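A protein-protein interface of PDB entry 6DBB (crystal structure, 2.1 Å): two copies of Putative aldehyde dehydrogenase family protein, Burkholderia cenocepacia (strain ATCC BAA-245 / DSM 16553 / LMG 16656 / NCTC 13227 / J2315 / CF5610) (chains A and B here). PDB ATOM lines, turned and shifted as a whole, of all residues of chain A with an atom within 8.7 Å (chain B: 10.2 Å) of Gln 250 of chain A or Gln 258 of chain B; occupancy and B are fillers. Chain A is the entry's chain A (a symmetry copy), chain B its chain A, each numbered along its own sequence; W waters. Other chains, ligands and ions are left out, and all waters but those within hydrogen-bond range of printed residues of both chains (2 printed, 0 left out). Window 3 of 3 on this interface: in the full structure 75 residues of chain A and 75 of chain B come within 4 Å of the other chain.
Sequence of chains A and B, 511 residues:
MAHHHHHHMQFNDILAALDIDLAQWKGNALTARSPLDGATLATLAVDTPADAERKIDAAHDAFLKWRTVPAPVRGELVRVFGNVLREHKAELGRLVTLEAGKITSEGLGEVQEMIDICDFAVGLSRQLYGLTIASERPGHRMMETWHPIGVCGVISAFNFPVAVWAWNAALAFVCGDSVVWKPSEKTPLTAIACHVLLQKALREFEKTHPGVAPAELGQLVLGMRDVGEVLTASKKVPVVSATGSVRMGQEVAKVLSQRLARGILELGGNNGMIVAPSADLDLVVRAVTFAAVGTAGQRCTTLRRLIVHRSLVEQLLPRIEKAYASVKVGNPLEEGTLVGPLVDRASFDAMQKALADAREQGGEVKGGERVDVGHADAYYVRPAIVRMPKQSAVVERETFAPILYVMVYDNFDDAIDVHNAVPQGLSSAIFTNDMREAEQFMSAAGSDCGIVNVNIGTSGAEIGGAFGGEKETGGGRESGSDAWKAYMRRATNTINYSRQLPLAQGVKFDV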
ATOM      1  N   ALA A 242       3.294  23.729 -24.455  1.00  0.00           N
ATOM      2  CA  ALA A 242       2.947  23.561 -25.862  1.00  0.00           C
ATOM      3  C   ALA A 242       1.684  24.344 -26.182  1.00  0.00           C
ATOM      4  O   ALA A 242       0.608  24.038 -25.662  1.00  0.00           O
ATOM      5  CB  ALA A 242       2.769  22.084 -26.220  1.00  0.00           C
ATOM      6  N   GLY A 244      -0.800  25.598 -29.286  1.00  0.00           N
ATOM      7  CA  GLY A 244      -1.144  25.286 -30.670  1.00  0.00           C
ATOM      8  C   GLY A 244      -2.495  24.612 -30.779  1.00  0.00           C
ATOM      9  O   GLY A 244      -3.355  24.758 -29.898  1.00  0.00           O
ATOM     10  N   SER A 245      -2.654  23.836 -31.851  1.00  0.00           N
ATOM     11  CA  SER A 245      -3.914  23.165 -32.136  1.00  0.00           C
ATOM     12  C   SER A 245      -4.181  22.038 -31.139  1.00  0.00           C
ATOM     13  O   SER A 245      -3.263  21.488 -30.517  1.00  0.00           O
ATOM     14  CB  SER A 245      -3.902  22.574 -33.547  1.00  0.00           C
ATOM     15  OG  SER A 245      -2.912  21.555 -33.615  1.00  0.00           O
ATOM     16  N   VAL A 246      -5.463  21.655 -31.041  1.00  0.00           N
ATOM     17  CA  VAL A 246      -5.844  20.511 -30.211  1.00  0.00           C
ATOM     18  C   VAL A 246      -5.071  19.268 -30.638  1.00  0.00           C
ATOM     19  O   VAL A 246      -4.590  18.495 -29.799  1.00  0.00           O
ATOM     20  CB  VAL A 246      -7.370  20.271 -30.280  1.00  0.00           C
ATOM     21  CG1 VAL A 246      -7.736  18.980 -29.578  1.00  0.00           C
ATOM     22  CG2 VAL A 246      -8.129  21.415 -29.659  1.00  0.00           C
ATOM     23  N   ARG A 247      -4.928  19.059 -31.951  1.00  0.00           N
ATOM     24  CA  ARG A 247      -4.264  17.848 -32.430  1.00  0.00           C
ATOM     25  C   ARG A 247      -2.795  17.830 -32.022  1.00  0.00           C
ATOM     26  O   ARG A 247      -2.260  16.777 -31.649  1.00  0.00           O
ATOM     27  CB  ARG A 247      -4.413  17.732 -33.954  1.00  0.00           C
ATOM     28  N   MET A 248      -2.113  18.972 -32.129  1.00  0.00           N
ATOM     29  CA  MET A 248      -0.740  19.059 -31.642  1.00  0.00           C
ATOM     30  C   MET A 248      -0.668  18.670 -30.176  1.00  0.00           C
ATOM     31  O   MET A 248       0.203  17.892 -29.766  1.00  0.00           O
ATOM     32  CB  MET A 248      -0.201  20.477 -31.842  1.00  0.00           C
ATOM     33  CG  MET A 248       1.197  20.738 -31.261  1.00  0.00           C
ATOM     34  SD  MET A 248       1.254  20.995 -29.478  1.00  0.00           S
ATOM     35  CE  MET A 248       0.354  22.541 -29.296  1.00  0.00           C
ATOM     36  N   GLY A 249      -1.580  19.219 -29.369  1.00  0.00           N
ATOM     37  CA  GLY A 249      -1.533  18.978 -27.939  1.00  0.00           C
ATOM     38  C   GLY A 249      -1.740  17.519 -27.594  1.00  0.00           C
ATOM     39  O   GLY A 249      -1.049  16.973 -26.732  1.00  0.00           O
ATOM     40  N   GLN A 250      -2.675  16.861 -28.279  1.00  0.00           N
ATOM     41  CA  GLN A 250      -2.868  15.429 -28.076  1.00  0.00           C
ATOM     42  C   GLN A 250      -1.596  14.647 -28.356  1.00  0.00           C
ATOM     43  O   GLN A 250      -1.199  13.783 -27.569  1.00  0.00           O
ATOM     44  CB  GLN A 250      -3.983  14.925 -28.979  1.00  0.00           C
ATOM     45  CG  GLN A 250      -5.361  15.383 -28.586  1.00  0.00           C
ATOM     46  CD  GLN A 250      -6.380  14.993 -29.642  1.00  0.00           C
ATOM     47  OE1 GLN A 250      -6.161  15.195 -30.842  1.00  0.00           O
ATOM     48  NE2 GLN A 250      -7.455  14.350 -29.208  1.00  0.00           N
ATOM     49  N   GLU A 251      -0.926  14.957 -29.467  1.00  0.00           N
ATOM     50  CA  GLU A 251       0.283  14.225 -29.817  1.00  0.00           C
ATOM     51  C   GLU A 251       1.404  14.507 -28.824  1.00  0.00           C
ATOM     52  O   GLU A 251       2.135  13.595 -28.425  1.00  0.00           O
ATOM     53  CB  GLU A 251       0.707  14.572 -31.251  1.00  0.00           C
ATOM     54  CG  GLU A 251      -0.252  14.043 -32.290  1.00  0.00           C
ATOM     55  CD  GLU A 251      -0.542  12.559 -32.084  1.00  0.00           C
ATOM     56  OE1 GLU A 251       0.434  11.778 -31.974  1.00  0.00           O
ATOM     57  OE2 GLU A 251      -1.738  12.178 -32.021  1.00  0.00           O
ATOM     58  N   VAL A 252       1.556  15.765 -28.409  1.00  0.00           N
ATOM     59  CA  VAL A 252       2.594  16.087 -27.443  1.00  0.00           C
ATOM     60  C   VAL A 252       2.307  15.401 -26.111  1.00  0.00           C
ATOM     61  O   VAL A 252       3.206  14.821 -25.489  1.00  0.00           O
ATOM     62  CB  VAL A 252       2.719  17.612 -27.289  1.00  0.00           C
ATOM     63  CG1 VAL A 252       3.692  17.942 -26.157  1.00  0.00           C
ATOM     64  CG2 VAL A 252       3.181  18.226 -28.614  1.00  0.00           C
ATOM     65  N   ALA A 253       1.053  15.454 -25.655  1.00  0.00           N
ATOM     66  CA  ALA A 253       0.704  14.865 -24.365  1.00  0.00           C
ATOM     67  C   ALA A 253       0.969  13.360 -24.357  1.00  0.00           C
ATOM     68  O   ALA A 253       1.422  12.807 -23.348  1.00  0.00           O
ATOM     69  CB  ALA A 253      -0.760  15.159 -24.034  1.00  0.00           C
ATOM     70  N   LYS A 254       0.717  12.684 -25.480  1.00  0.00           N
ATOM     71  CA  LYS A 254       1.026  11.259 -25.569  1.00  0.00           C
ATOM     72  C   LYS A 254       2.523  11.013 -25.369  1.00  0.00           C
ATOM     73  O   LYS A 254       2.920  10.146 -24.583  1.00  0.00           O
ATOM     74  CB  LYS A 254       0.546  10.706 -26.913  1.00  0.00           C
ATOM     75  N   VAL A 255       3.373  11.801 -26.033  1.00  0.00           N
ATOM     76  CA  VAL A 255       4.822  11.620 -25.861  1.00  0.00           C
ATOM     77  C   VAL A 255       5.253  11.943 -24.432  1.00  0.00           C
ATOM     78  O   VAL A 255       6.047  11.208 -23.828  1.00  0.00           O
ATOM     79  CB  VAL A 255       5.586  12.467 -26.896  1.00  0.00           C
ATOM     80  CG1 VAL A 255       7.102  12.496 -26.573  1.00  0.00           C
ATOM     81  CG2 VAL A 255       5.317  11.916 -28.304  1.00  0.00           C
ATOM     82  N   LEU A 256       4.754  13.046 -23.866  1.00  0.00           N
ATOM     83  CA  LEU A 256       5.083  13.367 -22.478  1.00  0.00           C
ATOM     84  C   LEU A 256       4.652  12.249 -21.532  1.00  0.00           C
ATOM     85  O   LEU A 256       5.397  11.873 -20.617  1.00  0.00           O
ATOM     86  CB  LEU A 256       4.418  14.686 -22.082  1.00  0.00           C
ATOM     87  CG  LEU A 256       4.854  15.940 -22.852  1.00  0.00           C
ATOM     88  CD1 LEU A 256       4.045  17.161 -22.411  1.00  0.00           C
ATOM     89  CD2 LEU A 256       6.349  16.185 -22.630  1.00  0.00           C
ATOM     90  N   SER A 257       3.454  11.698 -21.748  1.00  0.00           N
ATOM     91  CA  SER A 257       2.938  10.654 -20.870  1.00  0.00           C
ATOM     92  C   SER A 257       3.839   9.436 -20.885  1.00  0.00           C
ATOM     93  O   SER A 257       4.106   8.838 -19.836  1.00  0.00           O
ATOM     94  CB  SER A 257       1.529  10.260 -21.300  1.00  0.00           C
ATOM     95  OG  SER A 257       0.637  11.296 -21.005  1.00  0.00           O
ATOM     96  N   LEU A 265      -0.352  22.569 -21.436  1.00  0.00           N
ATOM     97  CA  LEU A 265      -1.022  22.480 -22.733  1.00  0.00           C
ATOM     98  C   LEU A 265      -1.954  23.671 -22.915  1.00  0.00           C
ATOM     99  O   LEU A 265      -2.893  23.858 -22.129  1.00  0.00           O
ATOM    100  CB  LEU A 265      -1.803  21.176 -22.866  1.00  0.00           C
ATOM    101  CG  LEU A 265      -0.948  19.929 -22.670  1.00  0.00           C
ATOM    102  CD1 LEU A 265      -1.806  18.674 -22.827  1.00  0.00           C
ATOM    103  CD2 LEU A 265       0.239  19.912 -23.620  1.00  0.00           C
ATOM    104  N   LEU A 267      -4.153  24.904 -25.833  1.00  0.00           N
ATOM    105  CA  LEU A 267      -4.607  24.474 -27.137  1.00  0.00           C
ATOM    106  C   LEU A 267      -5.725  25.404 -27.641  1.00  0.00           C
ATOM    107  O   LEU A 267      -5.816  26.572 -27.226  1.00  0.00           O
ATOM    108  CB  LEU A 267      -5.006  22.998 -27.043  1.00  0.00           C
ATOM    109  CG  LEU A 267      -3.947  22.160 -26.295  1.00  0.00           C
ATOM    110  CD1 LEU A 267      -4.355  20.682 -26.214  1.00  0.00           C
ATOM    111  CD2 LEU A 267      -2.566  22.273 -26.949  1.00  0.00           C
ATOM    112  N   GLU A 472     -10.942  20.520 -24.245  1.00  0.00           N
ATOM    113  CA  GLU A 472      -9.901  20.320 -25.240  1.00  0.00           C
ATOM    114  C   GLU A 472      -8.855  21.432 -25.245  1.00  0.00           C
ATOM    115  O   GLU A 472      -7.823  21.279 -25.901  1.00  0.00           O
ATOM    116  CB  GLU A 472     -10.533  20.178 -26.627  1.00  0.00           C
ATOM    117  CG  GLU A 472     -11.152  18.794 -26.877  1.00  0.00           C
ATOM    118  CD  GLU A 472     -11.573  18.586 -28.335  1.00  0.00           C
ATOM    119  OE1 GLU A 472     -11.538  19.553 -29.127  1.00  0.00           O
ATOM    120  OE2 GLU A 472     -11.930  17.454 -28.683  1.00  0.00           O
ATOM    121  N   THR A 473      -9.075  22.539 -24.528  1.00  0.00           N
ATOM    122  CA  THR A 473      -8.022  23.550 -24.468  1.00  0.00           C
ATOM    123  C   THR A 473      -6.802  23.049 -23.700  1.00  0.00           C
ATOM    124  O   THR A 473      -5.717  23.624 -23.846  1.00  0.00           O
ATOM    125  CB  THR A 473      -8.588  24.867 -23.911  1.00  0.00           C
ATOM    126  OG1 THR A 473      -9.701  25.265 -24.722  1.00  0.00           O
ATOM    127  CG2 THR A 473      -7.561  25.999 -23.949  1.00  0.00           C
ATOM    128  N   GLY A 474      -6.933  21.970 -22.915  1.00  0.00           N
ATOM    129  CA  GLY A 474      -5.772  21.240 -22.430  1.00  0.00           C
ATOM    130  C   GLY A 474      -5.384  21.455 -20.971  1.00  0.00           C
ATOM    131  O   GLY A 474      -4.528  20.717 -20.468  1.00  0.00           O
ATOM    132  N   THR B 232     -10.869   4.813 -17.138  1.00  0.00           N
ATOM    133  CA  THR B 232      -9.854   5.758 -17.599  1.00  0.00           C
ATOM    134  C   THR B 232     -10.229   6.367 -18.947  1.00  0.00           C
ATOM    135  O   THR B 232      -9.887   7.525 -19.216  1.00  0.00           O
ATOM    136  CB  THR B 232      -8.472   5.097 -17.673  1.00  0.00           C
ATOM    137  OG1 THR B 232      -8.520   3.990 -18.573  1.00  0.00           O
ATOM    138  CG2 THR B 232      -8.015   4.595 -16.293  1.00  0.00           C
ATOM    139  N   ALA B 233     -10.945   5.622 -19.792  1.00  0.00           N
ATOM    140  CA  ALA B 233     -11.339   6.125 -21.101  1.00  0.00           C
ATOM    141  C   ALA B 233     -12.608   6.972 -21.078  1.00  0.00           C
ATOM    142  O   ALA B 233     -12.895   7.643 -22.075  1.00  0.00           O
ATOM    143  CB  ALA B 233     -11.538   4.957 -22.075  1.00  0.00           C
ATOM    144  N   SER B 234     -13.349   7.012 -19.972  1.00  0.00           N
ATOM    145  CA  SER B 234     -14.652   7.676 -19.987  1.00  0.00           C
ATOM    146  C   SER B 234     -14.533   9.182 -20.158  1.00  0.00           C
ATOM    147  O   SER B 234     -13.903   9.861 -19.346  1.00  0.00           O
ATOM    148  CB  SER B 234     -15.421   7.391 -18.703  1.00  0.00           C
ATOM    149  OG  SER B 234     -16.536   8.270 -18.628  1.00  0.00           O
ATOM    150  N   LYS B 235     -15.231   9.715 -21.169  1.00  0.00           N
ATOM    151  CA  LYS B 235     -15.238  11.153 -21.411  1.00  0.00           C
ATOM    152  C   LYS B 235     -15.991  11.933 -20.337  1.00  0.00           C
ATOM    153  O   LYS B 235     -15.953  13.161 -20.370  1.00  0.00           O
ATOM    154  CB  LYS B 235     -15.831  11.459 -22.792  1.00  0.00           C
ATOM    155  N   GLN B 250       1.964   4.839 -16.683  1.00  0.00           N
ATOM    156  CA  GLN B 250       2.219   5.135 -18.089  1.00  0.00           C
ATOM    157  C   GLN B 250       1.006   4.835 -18.954  1.00  0.00           C
ATOM    158  O   GLN B 250       0.613   5.650 -19.794  1.00  0.00           O
ATOM    159  CB  GLN B 250       3.406   4.321 -18.581  1.00  0.00           C
ATOM    160  CG  GLN B 250       4.735   4.758 -18.027  1.00  0.00           C
ATOM    161  CD  GLN B 250       5.829   3.781 -18.418  1.00  0.00           C
ATOM    162  OE1 GLN B 250       5.666   2.561 -18.296  1.00  0.00           O
ATOM    163  NE2 GLN B 250       6.911   4.307 -18.977  1.00  0.00           N
ATOM    164  N   GLU B 251       0.383   3.675 -18.744  1.00  0.00           N
ATOM    165  CA  GLU B 251      -0.765   3.306 -19.559  1.00  0.00           C
ATOM    166  C   GLU B 251      -1.952   4.222 -19.284  1.00  0.00           C
ATOM    167  O   GLU B 251      -2.655   4.635 -20.212  1.00  0.00           O
ATOM    168  CB  GLU B 251      -1.128   1.834 -19.316  1.00  0.00           C
ATOM    169  CG  GLU B 251      -0.087   0.879 -19.849  1.00  0.00           C
ATOM    170  CD  GLU B 251       0.268   1.186 -21.301  1.00  0.00           C
ATOM    171  OE1 GLU B 251      -0.670   1.291 -22.127  1.00  0.00           O
ATOM    172  OE2 GLU B 251       1.477   1.333 -21.611  1.00  0.00           O
ATOM    173  N   VAL B 252      -2.192   4.554 -18.015  1.00  0.00           N
ATOM    174  CA  VAL B 252      -3.297   5.444 -17.698  1.00  0.00           C
ATOM    175  C   VAL B 252      -3.048   6.827 -18.292  1.00  0.00           C
ATOM    176  O   VAL B 252      -3.948   7.435 -18.885  1.00  0.00           O
ATOM    177  CB  VAL B 252      -3.508   5.502 -16.175  1.00  0.00           C
ATOM    178  CG1 VAL B 252      -4.558   6.561 -15.837  1.00  0.00           C
ATOM    179  CG2 VAL B 252      -3.928   4.121 -15.662  1.00  0.00           C
ATOM    180  N   ALA B 253      -1.825   7.343 -18.144  1.00  0.00           N
ATOM    181  CA  ALA B 253      -1.517   8.682 -18.641  1.00  0.00           C
ATOM    182  C   ALA B 253      -1.704   8.764 -20.156  1.00  0.00           C
ATOM    183  O   ALA B 253      -2.182   9.779 -20.675  1.00  0.00           O
ATOM    184  CB  ALA B 253      -0.091   9.071 -18.249  1.00  0.00           C
ATOM    185  N   LYS B 254      -1.356   7.697 -20.878  1.00  0.00           N
ATOM    186  CA  LYS B 254      -1.586   7.676 -22.321  1.00  0.00           C
ATOM    187  C   LYS B 254      -3.076   7.812 -22.637  1.00  0.00           C
ATOM    188  O   LYS B 254      -3.470   8.626 -23.479  1.00  0.00           O
ATOM    189  CB  LYS B 254      -1.004   6.393 -22.921  1.00  0.00           C
ATOM    190  N   VAL B 255      -3.928   7.061 -21.934  1.00  0.00           N
ATOM    191  CA  VAL B 255      -5.373   7.167 -22.186  1.00  0.00           C
ATOM    192  C   VAL B 255      -5.898   8.551 -21.807  1.00  0.00           C
ATOM    193  O   VAL B 255      -6.685   9.155 -22.550  1.00  0.00           O
ATOM    194  CB  VAL B 255      -6.122   6.047 -21.440  1.00  0.00           C
ATOM    195  CG1 VAL B 255      -7.653   6.288 -21.476  1.00  0.00           C
ATOM    196  CG2 VAL B 255      -5.748   4.689 -22.053  1.00  0.00           C
ATOM    197  N   LEU B 256      -5.489   9.076 -20.649  1.00  0.00           N
ATOM    198  CA  LEU B 256      -5.910  10.424 -20.270  1.00  0.00           C
ATOM    199  C   LEU B 256      -5.474  11.455 -21.308  1.00  0.00           C
ATOM    200  O   LEU B 256      -6.247  12.351 -21.673  1.00  0.00           O
ATOM    201  CB  LEU B 256      -5.337  10.776 -18.896  1.00  0.00           C
ATOM    202  CG  LEU B 256      -5.794   9.913 -17.713  1.00  0.00           C
ATOM    203  CD1 LEU B 256      -5.075  10.323 -16.427  1.00  0.00           C
ATOM    204  CD2 LEU B 256      -7.310  10.042 -17.539  1.00  0.00           C
ATOM    205  N   SER B 257      -4.239  11.334 -21.803  1.00  0.00           N
ATOM    206  CA  SER B 257      -3.718  12.297 -22.767  1.00  0.00           C
ATOM    207  C   SER B 257      -4.553  12.307 -24.032  1.00  0.00           C
ATOM    208  O   SER B 257      -4.846  13.373 -24.584  1.00  0.00           O
ATOM    209  CB  SER B 257      -2.269  11.964 -23.107  1.00  0.00           C
ATOM    210  OG  SER B 257      -1.450  12.244 -22.009  1.00  0.00           O
ATOM    211  N   GLN B 258      -4.965  11.127 -24.494  1.00  0.00           N
ATOM    212  CA  GLN B 258      -5.702  11.048 -25.750  1.00  0.00           C
ATOM    213  C   GLN B 258      -7.005  11.826 -25.682  1.00  0.00           C
ATOM    214  O   GLN B 258      -7.446  12.386 -26.691  1.00  0.00           O
ATOM    215  CB  GLN B 258      -5.958   9.589 -26.124  1.00  0.00           C
ATOM    216  CG  GLN B 258      -6.617   9.437 -27.479  1.00  0.00           C
ATOM    217  CD  GLN B 258      -5.954  10.314 -28.542  1.00  0.00           C
ATOM    218  OE1 GLN B 258      -4.747  10.213 -28.787  1.00  0.00           O
ATOM    219  NE2 GLN B 258      -6.740  11.189 -29.165  1.00  0.00           N
ATOM    220  N   ARG B 259      -7.616  11.923 -24.501  1.00  0.00           N
ATOM    221  CA  ARG B 259      -8.821  12.726 -24.351  1.00  0.00           C
ATOM    222  C   ARG B 259      -8.567  14.009 -23.553  1.00  0.00           C
ATOM    223  O   ARG B 259      -9.513  14.651 -23.082  1.00  0.00           O
ATOM    224  CB  ARG B 259      -9.931  11.871 -23.734  1.00  0.00           C
ATOM    225  CG  ARG B 259      -9.645  11.318 -22.328  1.00  0.00           C
ATOM    226  CD  ARG B 259     -10.747  10.333 -21.905  1.00  0.00           C
ATOM    227  NE  ARG B 259     -10.596   9.820 -20.538  1.00  0.00           N
ATOM    228  CZ  ARG B 259     -10.979  10.509 -19.465  1.00  0.00           C
ATOM    229  NH1 ARG B 259     -11.501  11.717 -19.634  1.00  0.00           N
ATOM    230  NH2 ARG B 259     -10.860   9.998 -18.240  1.00  0.00           N
ATOM    231  N   LEU B 260      -7.302  14.393 -23.408  1.00  0.00           N
ATOM    232  CA  LEU B 260      -6.898  15.654 -22.773  1.00  0.00           C
ATOM    233  C   LEU B 260      -7.500  15.812 -21.380  1.00  0.00           C
ATOM    234  O   LEU B 260      -8.027  16.864 -21.015  1.00  0.00           O
ATOM    235  CB  LEU B 260      -7.253  16.847 -23.664  1.00  0.00           C
ATOM    236  CG  LEU B 260      -6.431  16.833 -24.957  1.00  0.00           C
ATOM    237  CD1 LEU B 260      -6.944  17.882 -25.924  1.00  0.00           C
ATOM    238  CD2 LEU B 260      -4.949  17.040 -24.647  1.00  0.00           C
ATOM    239  N   ALA B 261      -7.414  14.750 -20.590  1.00  0.00           N
ATOM    240  CA  ALA B 261      -7.958  14.751 -19.242  1.00  0.00           C
ATOM    241  C   ALA B 261      -6.820  14.797 -18.232  1.00  0.00           C
ATOM    242  O   ALA B 261      -5.641  14.641 -18.569  1.00  0.00           O
ATOM    243  CB  ALA B 261      -8.852  13.533 -19.010  1.00  0.00           C
ATOM    244  N   ARG B 262      -7.180  15.034 -16.983  1.00  0.00           N
ATOM    245  CA  ARG B 262      -6.191  15.305 -15.956  1.00  0.00           C
ATOM    246  C   ARG B 262      -5.869  14.040 -15.170  1.00  0.00           C
ATOM    247  O   ARG B 262      -6.769  13.269 -14.821  1.00  0.00           O
ATOM    248  CB  ARG B 262      -6.700  16.393 -15.014  1.00  0.00           C
ATOM    249  CG  ARG B 262      -5.708  16.741 -13.912  1.00  0.00           C
ATOM    250  CD  ARG B 262      -6.352  17.644 -12.884  1.00  0.00           C
ATOM    251  NE  ARG B 262      -6.775  18.909 -13.478  1.00  0.00           N
ATOM    252  CZ  ARG B 262      -7.600  19.763 -12.879  1.00  0.00           C
ATOM    253  NH1 ARG B 262      -8.107  19.479 -11.675  1.00  0.00           N
ATOM    254  NH2 ARG B 262      -7.915  20.898 -13.483  1.00  0.00           N
ATOM    255  N   GLY B 263      -4.589  13.846 -14.878  1.00  0.00           N
ATOM    256  CA  GLY B 263      -4.136  12.727 -14.061  1.00  0.00           C
ATOM    257  C   GLY B 263      -3.517  13.186 -12.755  1.00  0.00           C
ATOM    258  O   GLY B 263      -2.824  14.201 -12.709  1.00  0.00           O
HETATM  259  O   HOH W   1     -10.880  17.195 -23.205  1.00  0.00           O
HETATM  260  O   HOH W   2      -8.010  19.725 -20.531  1.00  0.00           O
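O of Ala 253 of chain A sits at hydrogen-bond distance from OG of Ser 257 of chain B, 3.2 Å away.
O of Ala 253 of chain B sits at hydrogen-bond distance from OG of Ser 257 of chain A (3.2 Å).
O of Gln 258 of chain B sits at hydrogen-bond distance from NE2 of Gln 250 of chain A (3.2 Å).
OG of Ser 257 of chain B lies within hydrogen-bond range of OG of Ser 257 of chain A (2.5 Å).
The backbone carbonyl oxygen (O) of Ala 253 of chain B is in hydrogen-bond range of the side-chain hydroxyl (OG) of Ser 257 of chain B.
The backbone carbonyl oxygen of Ala 253 of chain A is in hydrogen-bond range of the side-chain hydroxyl of Ser 257 of chain A, at 2.9 Å.
The backbone NH (N) of Leu 267 of chain A lies within hydrogen-bond range of the backbone carbonyl oxygen (O) of Thr 473 of chain A (2.8 Å).
Among the printed residues, merely in contact across the chains: Val 246 of chain A with Leu 260 of chain B (3.9 Å), Gln 250 of chain A with Leu 260 of chain B (3.98 Å), Lys 254 of chain A with Ser 257 of chain B (3.9 Å), Ser 257 of chain A with Lys 254 of chain B (3.9 Å), Leu 265 of chain A with Leu 260 of chain B (3.98 Å), Leu 267 of chain A with Leu 260 of chain B (3.8 Å) and Glu 472 of chain A with Leu 260 of chain B (3.5 Å).
Of chain B, only Gln 258 and Leu 260 come within 4 Å of Gln 250 of chain A.
Of the printed residues of chain A, Gln 258 of chain B touches Gln 250 (3.2 Å).
No residue of chain B comes within 4 Å of Arg 247 of chain A.
No residue of chain B comes within 4 Å of Gly 249 of chain A.
No residue of chain B comes within 4 Å of Glu 251 of chain A.
Of chain B, only Ser 257 (3.2 Å) comes within 4 Å of Ala 253 of chain A.
Ser 257 of chain B touches three residues of chain A.
Printed residues of chain B within 4 Å of Leu 267 of chain A: Leu 260 (3.8 Å).
Printed residues of chain A within 4 Å of Lys 254 of chain B: Ser 257 (3.9 Å).
Of the printed residues of chain B, Glu 472 of chain A touches Leu 260.
Of the printed residues of chain B, Leu 265 of chain A touches Leu 260 (3.98 Å).
The nearest residue of chain B that does not touch Gln 250 of chain A is Ser 257 of chain B (4.5 Å).
Hydrophobic or aromatic side chains of chain A that line the printed part of chain B: Val 246, Ala 253, Leu 265 and Leu 267.
Printed residues of chain B that touch a printed residue of chain A: Ala 253, Lys 254, Ser 257, Gln 258 and Leu 260.
Among the printed residues, no Asp or Glu carboxylate lies within 4 Å of a Lys or Arg side-chain nitrogen of the other chain.
Ala 253 of chain A touches Ser 257 of chain B, and with the chains exchanged Ser 257 of chain A touches Ala 253 of chain B.
Lys 254 of chain A touches Ser 257 of chain B, and with the chains exchanged Ser 257 of chain A touches Lys 254 of chain B.
Ser 257 of chain A touches its own counterpart, Ser 257 of chain B.
Of the 11 pairs that touch across the chains among the printed residues, 5 have their exchanged pair printed and touching as well.
Water W1 bridges the backbone carbonyl oxygen of Arg 259 of chain B (2.9 Å) and the backbone NH of Glu 472 of chain A (3.5 Å).
Water W2 lies within hydrogen-bond range of O of Leu 260 of chain B (2.9 Å) and N of Gly 474 of chain A (3.4 Å).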
